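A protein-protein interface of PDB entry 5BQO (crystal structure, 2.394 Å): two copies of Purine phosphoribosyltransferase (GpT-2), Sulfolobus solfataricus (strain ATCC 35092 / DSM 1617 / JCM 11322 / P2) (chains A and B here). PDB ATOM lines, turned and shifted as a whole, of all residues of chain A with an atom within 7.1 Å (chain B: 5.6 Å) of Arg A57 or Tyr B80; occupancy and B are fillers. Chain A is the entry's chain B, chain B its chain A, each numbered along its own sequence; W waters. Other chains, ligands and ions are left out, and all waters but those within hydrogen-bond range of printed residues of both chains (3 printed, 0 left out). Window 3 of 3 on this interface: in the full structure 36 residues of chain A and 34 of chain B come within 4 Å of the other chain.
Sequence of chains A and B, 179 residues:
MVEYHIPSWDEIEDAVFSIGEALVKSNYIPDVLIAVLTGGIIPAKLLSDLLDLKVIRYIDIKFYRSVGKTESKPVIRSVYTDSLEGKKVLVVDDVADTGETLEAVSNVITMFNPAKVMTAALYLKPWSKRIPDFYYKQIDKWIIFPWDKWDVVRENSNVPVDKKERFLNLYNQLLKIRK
Among the printed residues, merely in contact across the chains: Leu A37 with Tyr B58, Ile A41 with Tyr B58, Arg A57 with Tyr B80, Tyr A58 with Leu B37, Tyr A80 with Arg B57 and Tyr A80 with Tyr B80.
Of chain B, only Tyr B80 comes within 4 Å of Arg A57. Of chain A, only Arg A57 (3.7 Å) and Tyr A80 (3.8 Å) come within 4 Å of Tyr B80. Of the printed residues of chain A, Tyr B58 touches Leu A37 and Ile A41. Printed residues of chain A within 4 Å of Arg B57: Tyr A80. Of the printed residues of chain A, Leu B37 touches Tyr A58 (3.2 Å). Ala A44 touches none of the printed residues of chain B. The nearest residue of chain B that does not touch Arg A57 is Asp B60 (4.4 Å). The nearest residue of chain A that does not touch Tyr B80 is Tyr A58 (4.1 Å).
Leu A37 touches Tyr B58, and with the chains exchanged Tyr A58 touches Leu B37. Arg A57 touches Tyr B80, and with the chains exchanged Tyr A80 touches Arg B57. Tyr A80 touches its own counterpart, Tyr B80. Of the 6 pairs that touch across the chains among the printed residues, 5 have their exchanged pair printed and touching as well.
Of the 21 printed residues of chain A, 5 touch a printed residue of chain B. Hydrophobic or aromatic side chains of chain A within 4 Å of the printed part of chain B: Leu A37, Ile A41, Tyr A58 and Tyr A80. Along chain A the printed residues that touch a printed residue of chain B span positions 37 to 80. Printed residues of chain B that touch a printed residue of chain A: Leu B37, Arg B57, Tyr B58 and Tyr B80.
N of Leu B37 lies within hydrogen-bond range of O of Ile B59 (3.0 Å). The guanidinium group (NE) of Arg B57 lies within salt-bridge range of the side-chain carboxylate (OD1) of Asp B82 (3.1 Å). The backbone carbonyl oxygen (O) of Tyr B58 sits at hydrogen-bond distance from the backbone NH (N) of Tyr B80 (2.8 Å). N of Arg A57 lies within hydrogen-bond range of O of Leu A33 (2.6 Å). O of Arg A57 lies within hydrogen-bond range of N of Ala A35 (2.8 Å). O of Ile A59 sits at hydrogen-bond distance from N of Leu A37, 3.0 Å away.
Water W1 bridges the side-chain hydroxyl (OH) of Tyr A80 and the backbone NH (N) of Asp B82. Water W2 lies within hydrogen-bond range of OH of Tyr A80 (2.8 Å) and NH2 of Arg B57 (3.3 Å). Water W3 lies within hydrogen-bond range of the side-chain hydroxyl (OH) of Tyr B80 (2.9 Å), the backbone NH (N) of Asp A82 (3.1 Å) and the guanidinium group (NE) of Arg A57 (3.4 Å).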
ATOM      1  N   VAL A  32     -25.585 -26.314  24.817  1.00  0.00           N
ATOM      2  CA  VAL A  32     -25.532 -25.003  25.454  1.00  0.00           C
ATOM      3  C   VAL A  32     -26.517 -24.919  26.617  1.00  0.00           C
ATOM      4  O   VAL A  32     -27.674 -25.321  26.491  1.00  0.00           O
ATOM      5  CB  VAL A  32     -25.849 -23.869  24.448  1.00  0.00           C
ATOM      6  CG1 VAL A  32     -25.913 -22.523  25.156  1.00  0.00           C
ATOM      7  CG2 VAL A  32     -24.822 -23.835  23.324  1.00  0.00           C
ATOM      8  N   LEU A  33     -26.052 -24.407  27.752  1.00  0.00           N
ATOM      9  CA  LEU A  33     -26.938 -24.089  28.865  1.00  0.00           C
ATOM     10  C   LEU A  33     -27.303 -22.611  28.837  1.00  0.00           C
ATOM     11  O   LEU A  33     -26.424 -21.748  28.826  1.00  0.00           O
ATOM     12  CB  LEU A  33     -26.291 -24.441  30.206  1.00  0.00           C
ATOM     13  CG  LEU A  33     -26.221 -25.913  30.609  1.00  0.00           C
ATOM     14  CD1 LEU A  33     -25.708 -26.043  32.036  1.00  0.00           C
ATOM     15  CD2 LEU A  33     -27.581 -26.578  30.462  1.00  0.00           C
ATOM     16  N   ILE A  34     -28.598 -22.318  28.814  1.00  0.00           N
ATOM     17  CA  ILE A  34     -29.053 -20.935  28.866  1.00  0.00           C
ATOM     18  C   ILE A  34     -29.703 -20.640  30.212  1.00  0.00           C
ATOM     19  O   ILE A  34     -30.784 -21.140  30.521  1.00  0.00           O
ATOM     20  CB  ILE A  34     -30.040 -20.613  27.734  1.00  0.00           C
ATOM     21  CG1 ILE A  34     -29.335 -20.726  26.381  1.00  0.00           C
ATOM     22  CG2 ILE A  34     -30.618 -19.218  27.910  1.00  0.00           C
ATOM     23  CD1 ILE A  34     -30.151 -20.215  25.225  1.00  0.00           C
ATOM     24  N   ALA A  35     -29.023 -19.825  31.012  1.00  0.00           N
ATOM     25  CA  ALA A  35     -29.494 -19.504  32.350  1.00  0.00           C
ATOM     26  C   ALA A  35     -30.442 -18.315  32.335  1.00  0.00           C
ATOM     27  O   ALA A  35     -30.187 -17.312  31.670  1.00  0.00           O
ATOM     28  CB  ALA A  35     -28.314 -19.225  33.269  1.00  0.00           C
ATOM     29  N   VAL A  36     -31.541 -18.438  33.069  1.00  0.00           N
ATOM     30  CA  VAL A  36     -32.452 -17.320  33.259  1.00  0.00           C
ATOM     31  C   VAL A  36     -31.923 -16.418  34.365  1.00  0.00           C
ATOM     32  O   VAL A  36     -31.844 -16.823  35.525  1.00  0.00           O
ATOM     33  CB  VAL A  36     -33.873 -17.790  33.612  1.00  0.00           C
ATOM     34  CG1 VAL A  36     -34.793 -16.594  33.807  1.00  0.00           C
ATOM     35  CG2 VAL A  36     -34.410 -18.708  32.525  1.00  0.00           C
ATOM     36  N   LEU A  37     -31.550 -15.198  34.000  1.00  0.00           N
ATOM     37  CA  LEU A  37     -31.014 -14.248  34.964  1.00  0.00           C
ATOM     38  C   LEU A  37     -32.135 -13.633  35.796  1.00  0.00           C
ATOM     39  O   LEU A  37     -33.140 -13.178  35.251  1.00  0.00           O
ATOM     40  CB  LEU A  37     -30.216 -13.154  34.253  1.00  0.00           C
ATOM     41  CG  LEU A  37     -29.024 -13.645  33.430  1.00  0.00           C
ATOM     42  CD1 LEU A  37     -28.307 -12.475  32.774  1.00  0.00           C
ATOM     43  CD2 LEU A  37     -28.067 -14.450  34.296  1.00  0.00           C
ATOM     44  N   ILE A  41     -29.202 -18.764  37.541  1.00  0.00           N
ATOM     45  CA  ILE A  41     -27.772 -18.737  37.253  1.00  0.00           C
ATOM     46  C   ILE A  41     -26.973 -19.619  38.217  1.00  0.00           C
ATOM     47  O   ILE A  41     -25.838 -19.997  37.925  1.00  0.00           O
ATOM     48  CB  ILE A  41     -27.217 -17.295  37.295  1.00  0.00           C
ATOM     49  CG1 ILE A  41     -25.949 -17.186  36.444  1.00  0.00           C
ATOM     50  CG2 ILE A  41     -26.975 -16.845  38.730  1.00  0.00           C
ATOM     51  CD1 ILE A  41     -25.321 -15.811  36.449  1.00  0.00           C
ATOM     52  N   ALA A  44     -27.922 -23.387  36.963  1.00  0.00           N
ATOM     53  CA  ALA A  44     -27.224 -23.611  35.700  1.00  0.00           C
ATOM     54  C   ALA A  44     -25.751 -23.932  35.928  1.00  0.00           C
ATOM     55  O   ALA A  44     -25.204 -24.841  35.306  1.00  0.00           O
ATOM     56  CB  ALA A  44     -27.367 -22.400  34.793  1.00  0.00           C
ATOM     57  N   LYS A  54     -19.685 -27.144  29.267  1.00  0.00           N
ATOM     58  CA  LYS A  54     -18.742 -26.030  29.311  1.00  0.00           C
ATOM     59  C   LYS A  54     -19.273 -24.737  28.695  1.00  0.00           C
ATOM     60  O   LYS A  54     -18.749 -23.657  28.968  1.00  0.00           O
ATOM     61  CB  LYS A  54     -17.439 -26.431  28.617  1.00  0.00           C
ATOM     62  CG  LYS A  54     -17.209 -27.932  28.579  1.00  0.00           C
ATOM     63  CD  LYS A  54     -15.939 -28.284  27.830  1.00  0.00           C
ATOM     64  CE  LYS A  54     -15.717 -29.788  27.812  1.00  0.00           C
ATOM     65  NZ  LYS A  54     -16.946 -30.518  27.392  1.00  0.00           N
ATOM     66  N   VAL A  55     -20.305 -24.842  27.866  1.00  0.00           N
ATOM     67  CA  VAL A  55     -20.879 -23.657  27.239  1.00  0.00           C
ATOM     68  C   VAL A  55     -22.132 -23.192  27.969  1.00  0.00           C
ATOM     69  O   VAL A  55     -23.155 -23.877  27.972  1.00  0.00           O
ATOM     70  CB  VAL A  55     -21.223 -23.906  25.759  1.00  0.00           C
ATOM     71  CG1 VAL A  55     -21.836 -22.657  25.145  1.00  0.00           C
ATOM     72  CG2 VAL A  55     -19.981 -24.321  24.991  1.00  0.00           C
ATOM     73  N   ILE A  56     -22.042 -22.021  28.591  1.00  0.00           N
ATOM     74  CA  ILE A  56     -23.184 -21.425  29.269  1.00  0.00           C
ATOM     75  C   ILE A  56     -23.483 -20.039  28.713  1.00  0.00           C
ATOM     76  O   ILE A  56     -22.596 -19.189  28.633  1.00  0.00           O
ATOM     77  CB  ILE A  56     -22.954 -21.307  30.785  1.00  0.00           C
ATOM     78  CG1 ILE A  56     -22.577 -22.661  31.386  1.00  0.00           C
ATOM     79  CG2 ILE A  56     -24.195 -20.752  31.467  1.00  0.00           C
ATOM     80  CD1 ILE A  56     -22.284 -22.596  32.867  1.00  0.00           C
ATOM     81  N   ARG A  57     -24.733 -19.818  28.324  1.00  0.00           N
ATOM     82  CA  ARG A  57     -25.170 -18.501  27.882  1.00  0.00           C
ATOM     83  C   ARG A  57     -26.302 -18.012  28.776  1.00  0.00           C
ATOM     84  O   ARG A  57     -26.804 -18.761  29.614  1.00  0.00           O
ATOM     85  CB  ARG A  57     -25.598 -18.533  26.415  1.00  0.00           C
ATOM     86  CG  ARG A  57     -24.458 -18.851  25.458  1.00  0.00           C
ATOM     87  CD  ARG A  57     -23.299 -17.881  25.644  1.00  0.00           C
ATOM     88  NE  ARG A  57     -22.226 -18.108  24.679  1.00  0.00           N
ATOM     89  CZ  ARG A  57     -21.129 -18.815  24.930  1.00  0.00           C
ATOM     90  NH1 ARG A  57     -20.952 -19.372  26.121  1.00  0.00           N
ATOM     91  NH2 ARG A  57     -20.207 -18.968  23.989  1.00  0.00           N
ATOM     92  N   TYR A  58     -26.693 -16.752  28.611  1.00  0.00           N
ATOM     93  CA  TYR A  58     -27.592 -16.116  29.567  1.00  0.00           C
ATOM     94  C   TYR A  58     -28.631 -15.227  28.894  1.00  0.00           C
ATOM     95  O   TYR A  58     -28.405 -14.707  27.802  1.00  0.00           O
ATOM     96  CB  TYR A  58     -26.782 -15.288  30.574  1.00  0.00           C
ATOM     97  CG  TYR A  58     -25.548 -15.996  31.089  1.00  0.00           C
ATOM     98  CD1 TYR A  58     -24.330 -15.886  30.425  1.00  0.00           C
ATOM     99  CD2 TYR A  58     -25.603 -16.786  32.228  1.00  0.00           C
ATOM    100  CE1 TYR A  58     -23.203 -16.539  30.885  1.00  0.00           C
ATOM    101  CE2 TYR A  58     -24.480 -17.441  32.698  1.00  0.00           C
ATOM    102  CZ  TYR A  58     -23.284 -17.314  32.023  1.00  0.00           C
ATOM    103  OH  TYR A  58     -22.165 -17.966  32.488  1.00  0.00           O
ATOM    104  N   ILE A  59     -29.772 -15.062  29.555  1.00  0.00           N
ATOM    105  CA  ILE A  59     -30.780 -14.114  29.105  1.00  0.00           C
ATOM    106  C   ILE A  59     -31.327 -13.307  30.283  1.00  0.00           C
ATOM    107  O   ILE A  59     -31.746 -13.861  31.301  1.00  0.00           O
ATOM    108  CB  ILE A  59     -31.940 -14.817  28.353  1.00  0.00           C
ATOM    109  CG1 ILE A  59     -32.982 -13.791  27.899  1.00  0.00           C
ATOM    110  CG2 ILE A  59     -32.572 -15.919  29.202  1.00  0.00           C
ATOM    111  CD1 ILE A  59     -34.082 -14.370  27.036  1.00  0.00           C
ATOM    112  N   VAL A  79     -30.214 -10.193  25.683  1.00  0.00           N
ATOM    113  CA  VAL A  79     -29.899 -11.589  25.398  1.00  0.00           C
ATOM    114  C   VAL A  79     -28.403 -11.758  25.138  1.00  0.00           C
ATOM    115  O   VAL A  79     -27.867 -11.217  24.171  1.00  0.00           O
ATOM    116  CB  VAL A  79     -30.689 -12.121  24.185  1.00  0.00           C
ATOM    117  CG1 VAL A  79     -30.370 -13.587  23.951  1.00  0.00           C
ATOM    118  CG2 VAL A  79     -32.183 -11.928  24.397  1.00  0.00           C
ATOM    119  N   TYR A  80     -27.738 -12.512  26.008  1.00  0.00           N
ATOM    120  CA  TYR A  80     -26.292 -12.690  25.931  1.00  0.00           C
ATOM    121  C   TYR A  80     -25.897 -14.026  25.309  1.00  0.00           C
ATOM    122  O   TYR A  80     -25.601 -14.980  26.029  1.00  0.00           O
ATOM    123  CB  TYR A  80     -25.671 -12.591  27.326  1.00  0.00           C
ATOM    124  CG  TYR A  80     -25.892 -11.271  28.023  1.00  0.00           C
ATOM    125  CD1 TYR A  80     -25.757 -10.068  27.342  1.00  0.00           C
ATOM    126  CD2 TYR A  80     -26.234 -11.226  29.368  1.00  0.00           C
ATOM    127  CE1 TYR A  80     -25.956  -8.860  27.981  1.00  0.00           C
ATOM    128  CE2 TYR A  80     -26.437 -10.024  30.016  1.00  0.00           C
ATOM    129  CZ  TYR A  80     -26.296  -8.844  29.317  1.00  0.00           C
ATOM    130  OH  TYR A  80     -26.497  -7.644  29.959  1.00  0.00           O
ATOM    131  N   THR A  81     -25.878 -14.097  23.981  1.00  0.00           N
ATOM    132  CA  THR A  81     -25.463 -15.325  23.308  1.00  0.00           C
ATOM    133  C   THR A  81     -25.092 -15.131  21.842  1.00  0.00           C
ATOM    134  O   THR A  81     -25.635 -14.266  21.151  1.00  0.00           O
ATOM    135  CB  THR A  81     -26.560 -16.408  23.384  1.00  0.00           C
ATOM    136  OG1 THR A  81     -26.091 -17.611  22.760  1.00  0.00           O
ATOM    137  CG2 THR A  81     -27.832 -15.941  22.691  1.00  0.00           C
ATOM    138  N   ASP A  82     -24.153 -15.947  21.380  1.00  0.00           N
ATOM    139  CA  ASP A  82     -23.823 -16.030  19.966  1.00  0.00           C
ATOM    140  C   ASP A  82     -24.797 -16.983  19.278  1.00  0.00           C
ATOM    141  O   ASP A  82     -25.854 -17.295  19.825  1.00  0.00           O
ATOM    142  CB  ASP A  82     -22.377 -16.491  19.776  1.00  0.00           C
ATOM    143  CG  ASP A  82     -21.944 -17.498  20.827  1.00  0.00           C
ATOM    144  OD1 ASP A  82     -22.824 -18.133  21.445  1.00  0.00           O
ATOM    145  OD2 ASP A  82     -20.722 -17.651  21.038  1.00  0.00           O
ATOM    146  N   SER A  83     -24.437 -17.446  18.084  1.00  0.00           N
ATOM    147  CA  SER A  83     -25.308 -18.322  17.306  1.00  0.00           C
ATOM    148  C   SER A  83     -25.639 -19.617  18.044  1.00  0.00           C
ATOM    149  O   SER A  83     -24.787 -20.197  18.717  1.00  0.00           O
ATOM    150  CB  SER A  83     -24.669 -18.647  15.955  1.00  0.00           C
ATOM    151  OG  SER A  83     -25.438 -19.602  15.247  1.00  0.00           O
ATOM    152  N   LEU A  84     -26.885 -20.061  17.910  1.00  0.00           N
ATOM    153  CA  LEU A  84     -27.334 -21.297  18.540  1.00  0.00           C
ATOM    154  C   LEU A  84     -27.866 -22.276  17.502  1.00  0.00           C
ATOM    155  O   LEU A  84     -28.486 -23.279  17.848  1.00  0.00           O
ATOM    156  CB  LEU A  84     -28.417 -21.009  19.582  1.00  0.00           C
ATOM    157  CG  LEU A  84     -28.027 -20.132  20.772  1.00  0.00           C
ATOM    158  CD1 LEU A  84     -29.226 -19.907  21.679  1.00  0.00           C
ATOM    159  CD2 LEU A  84     -26.874 -20.756  21.543  1.00  0.00           C
ATOM    160  N   LEU A  90     -30.642 -26.181  26.516  1.00  0.00           N
ATOM    161  CA  LEU A  90     -31.431 -26.327  27.733  1.00  0.00           C
ATOM    162  C   LEU A  90     -31.564 -24.987  28.447  1.00  0.00           C
ATOM    163  O   LEU A  90     -30.568 -24.308  28.700  1.00  0.00           O
ATOM    164  CB  LEU A  90     -30.805 -27.363  28.668  1.00  0.00           C
ATOM    165  CG  LEU A  90     -31.574 -27.647  29.961  1.00  0.00           C
ATOM    166  CD1 LEU A  90     -32.944 -28.236  29.657  1.00  0.00           C
ATOM    167  CD2 LEU A  90     -30.780 -28.566  30.877  1.00  0.00           C
ATOM    168  N   LEU B  37     -17.064 -15.000  34.872  1.00  0.00           N
ATOM    169  CA  LEU B  37     -17.586 -16.301  34.478  1.00  0.00           C
ATOM    170  C   LEU B  37     -16.481 -17.354  34.478  1.00  0.00           C
ATOM    171  O   LEU B  37     -15.419 -17.144  33.894  1.00  0.00           O
ATOM    172  CB  LEU B  37     -18.242 -16.217  33.100  1.00  0.00           C
ATOM    173  CG  LEU B  37     -19.406 -15.231  32.985  1.00  0.00           C
ATOM    174  CD1 LEU B  37     -19.922 -15.169  31.556  1.00  0.00           C
ATOM    175  CD2 LEU B  37     -20.524 -15.597  33.948  1.00  0.00           C
ATOM    176  N   ARG B  57     -23.657  -7.453  35.876  1.00  0.00           N
ATOM    177  CA  ARG B  57     -23.175  -7.725  34.528  1.00  0.00           C
ATOM    178  C   ARG B  57     -22.068  -8.772  34.586  1.00  0.00           C
ATOM    179  O   ARG B  57     -21.611  -9.135  35.669  1.00  0.00           O
ATOM    180  CB  ARG B  57     -22.688  -6.442  33.853  1.00  0.00           C
ATOM    181  CG  ARG B  57     -23.793  -5.422  33.617  1.00  0.00           C
ATOM    182  CD  ARG B  57     -24.951  -6.036  32.839  1.00  0.00           C
ATOM    183  NE  ARG B  57     -25.994  -5.060  32.537  1.00  0.00           N
ATOM    184  CZ  ARG B  57     -27.089  -4.881  33.269  1.00  0.00           C
ATOM    185  NH1 ARG B  57     -27.294  -5.614  34.355  1.00  0.00           N
ATOM    186  NH2 ARG B  57     -27.983  -3.967  32.914  1.00  0.00           N
ATOM    187  N   TYR B  58     -21.642  -9.263  33.426  1.00  0.00           N
ATOM    188  CA  TYR B  58     -20.781 -10.441  33.385  1.00  0.00           C
ATOM    189  C   TYR B  58     -19.650 -10.323  32.368  1.00  0.00           C
ATOM    190  O   TYR B  58     -19.740  -9.558  31.409  1.00  0.00           O
ATOM    191  CB  TYR B  58     -21.621 -11.685  33.077  1.00  0.00           C
ATOM    192  CG  TYR B  58     -22.907 -11.758  33.873  1.00  0.00           C
ATOM    193  CD1 TYR B  58     -24.081 -11.197  33.385  1.00  0.00           C
ATOM    194  CD2 TYR B  58     -22.943 -12.377  35.115  1.00  0.00           C
ATOM    195  CE1 TYR B  58     -25.254 -11.252  34.111  1.00  0.00           C
ATOM    196  CE2 TYR B  58     -24.114 -12.439  35.847  1.00  0.00           C
ATOM    197  CZ  TYR B  58     -25.266 -11.876  35.340  1.00  0.00           C
ATOM    198  OH  TYR B  58     -26.434 -11.935  36.066  1.00  0.00           O
ATOM    199  N   ILE B  59     -18.586 -11.088  32.590  1.00  0.00           N
ATOM    200  CA  ILE B  59     -17.474 -11.146  31.648  1.00  0.00           C
ATOM    201  C   ILE B  59     -16.963 -12.580  31.498  1.00  0.00           C
ATOM    202  O   ILE B  59     -16.741 -13.285  32.485  1.00  0.00           O
ATOM    203  CB  ILE B  59     -16.316 -10.204  32.074  1.00  0.00           C
ATOM    204  CG1 ILE B  59     -15.176 -10.254  31.054  1.00  0.00           C
ATOM    205  CG2 ILE B  59     -15.821 -10.530  33.481  1.00  0.00           C
ATOM    206  CD1 ILE B  59     -14.021  -9.334  31.383  1.00  0.00           C
ATOM    207  N   ASP B  60     -16.804 -13.013  30.253  1.00  0.00           N
ATOM    208  CA  ASP B  60     -16.326 -14.358  29.958  1.00  0.00           C
ATOM    209  C   ASP B  60     -14.819 -14.334  29.741  1.00  0.00           C
ATOM    210  O   ASP B  60     -14.347 -14.089  28.631  1.00  0.00           O
ATOM    211  CB  ASP B  60     -17.041 -14.924  28.726  1.00  0.00           C
ATOM    212  CG  ASP B  60     -16.838 -16.422  28.560  1.00  0.00           C
ATOM    213  OD1 ASP B  60     -15.836 -16.965  29.072  1.00  0.00           O
ATOM    214  OD2 ASP B  60     -17.687 -17.061  27.903  1.00  0.00           O
ATOM    215  N   SER B  78     -15.802 -12.821  25.755  1.00  0.00           N
ATOM    216  CA  SER B  78     -16.895 -11.880  25.528  1.00  0.00           C
ATOM    217  C   SER B  78     -17.101 -10.992  26.750  1.00  0.00           C
ATOM    218  O   SER B  78     -16.746 -11.366  27.867  1.00  0.00           O
ATOM    219  CB  SER B  78     -18.193 -12.620  25.197  1.00  0.00           C
ATOM    220  OG  SER B  78     -18.531 -13.543  26.216  1.00  0.00           O
ATOM    221  N   VAL B  79     -17.672  -9.811  26.531  1.00  0.00           N
ATOM    222  CA  VAL B  79     -17.998  -8.901  27.623  1.00  0.00           C
ATOM    223  C   VAL B  79     -19.487  -8.582  27.608  1.00  0.00           C
ATOM    224  O   VAL B  79     -19.994  -7.996  26.651  1.00  0.00           O
ATOM    225  CB  VAL B  79     -17.197  -7.589  27.539  1.00  0.00           C
ATOM    226  CG1 VAL B  79     -17.469  -6.730  28.762  1.00  0.00           C
ATOM    227  CG2 VAL B  79     -15.710  -7.879  27.409  1.00  0.00           C
ATOM    228  N   TYR B  80     -20.185  -8.967  28.672  1.00  0.00           N
ATOM    229  CA  TYR B  80     -21.634  -8.804  28.739  1.00  0.00           C
ATOM    230  C   TYR B  80     -22.046  -7.623  29.610  1.00  0.00           C
ATOM    231  O   TYR B  80     -22.506  -7.812  30.736  1.00  0.00           O
ATOM    232  CB  TYR B  80     -22.287 -10.079  29.275  1.00  0.00           C
ATOM    233  CG  TYR B  80     -22.088 -11.302  28.409  1.00  0.00           C
ATOM    234  CD1 TYR B  80     -22.087 -11.207  27.024  1.00  0.00           C
ATOM    235  CD2 TYR B  80     -21.901 -12.554  28.980  1.00  0.00           C
ATOM    236  CE1 TYR B  80     -21.907 -12.326  26.231  1.00  0.00           C
ATOM    237  CE2 TYR B  80     -21.719 -13.677  28.198  1.00  0.00           C
ATOM    238  CZ  TYR B  80     -21.722 -13.558  26.824  1.00  0.00           C
ATOM    239  OH  TYR B  80     -21.541 -14.677  26.046  1.00  0.00           O
ATOM    240  N   THR B  81     -21.893  -6.408  29.094  1.00  0.00           N
ATOM    241  CA  THR B  81     -22.293  -5.224  29.847  1.00  0.00           C
ATOM    242  C   THR B  81     -22.604  -4.027  28.955  1.00  0.00           C
ATOM    243  O   THR B  81     -22.119  -3.925  27.828  1.00  0.00           O
ATOM    244  CB  THR B  81     -21.206  -4.806  30.857  1.00  0.00           C
ATOM    245  OG1 THR B  81     -21.678  -3.699  31.637  1.00  0.00           O
ATOM    246  CG2 THR B  81     -19.930  -4.402  30.136  1.00  0.00           C
ATOM    247  N   ASP B  82     -23.428  -3.125  29.477  1.00  0.00           N
ATOM    248  CA  ASP B  82     -23.706  -1.859  28.817  1.00  0.00           C
ATOM    249  C   ASP B  82     -22.817  -0.771  29.410  1.00  0.00           C
ATOM    250  O   ASP B  82     -21.774  -1.068  29.994  1.00  0.00           O
ATOM    251  CB  ASP B  82     -25.185  -1.491  28.946  1.00  0.00           C
ATOM    252  CG  ASP B  82     -25.716  -1.686  30.354  1.00  0.00           C
ATOM    253  OD1 ASP B  82     -25.100  -2.454  31.124  1.00  0.00           O
ATOM    254  OD2 ASP B  82     -26.753  -1.076  30.689  1.00  0.00           O
HETATM  255  O   HOH W   1     -25.948  -5.284  28.902  1.00  0.00           O
HETATM  256  O   HOH W   2     -28.881  -6.599  31.066  1.00  0.00           O
HETATM  257  O   HOH W   3     -21.738 -15.119  23.224  1.00  0.00           O
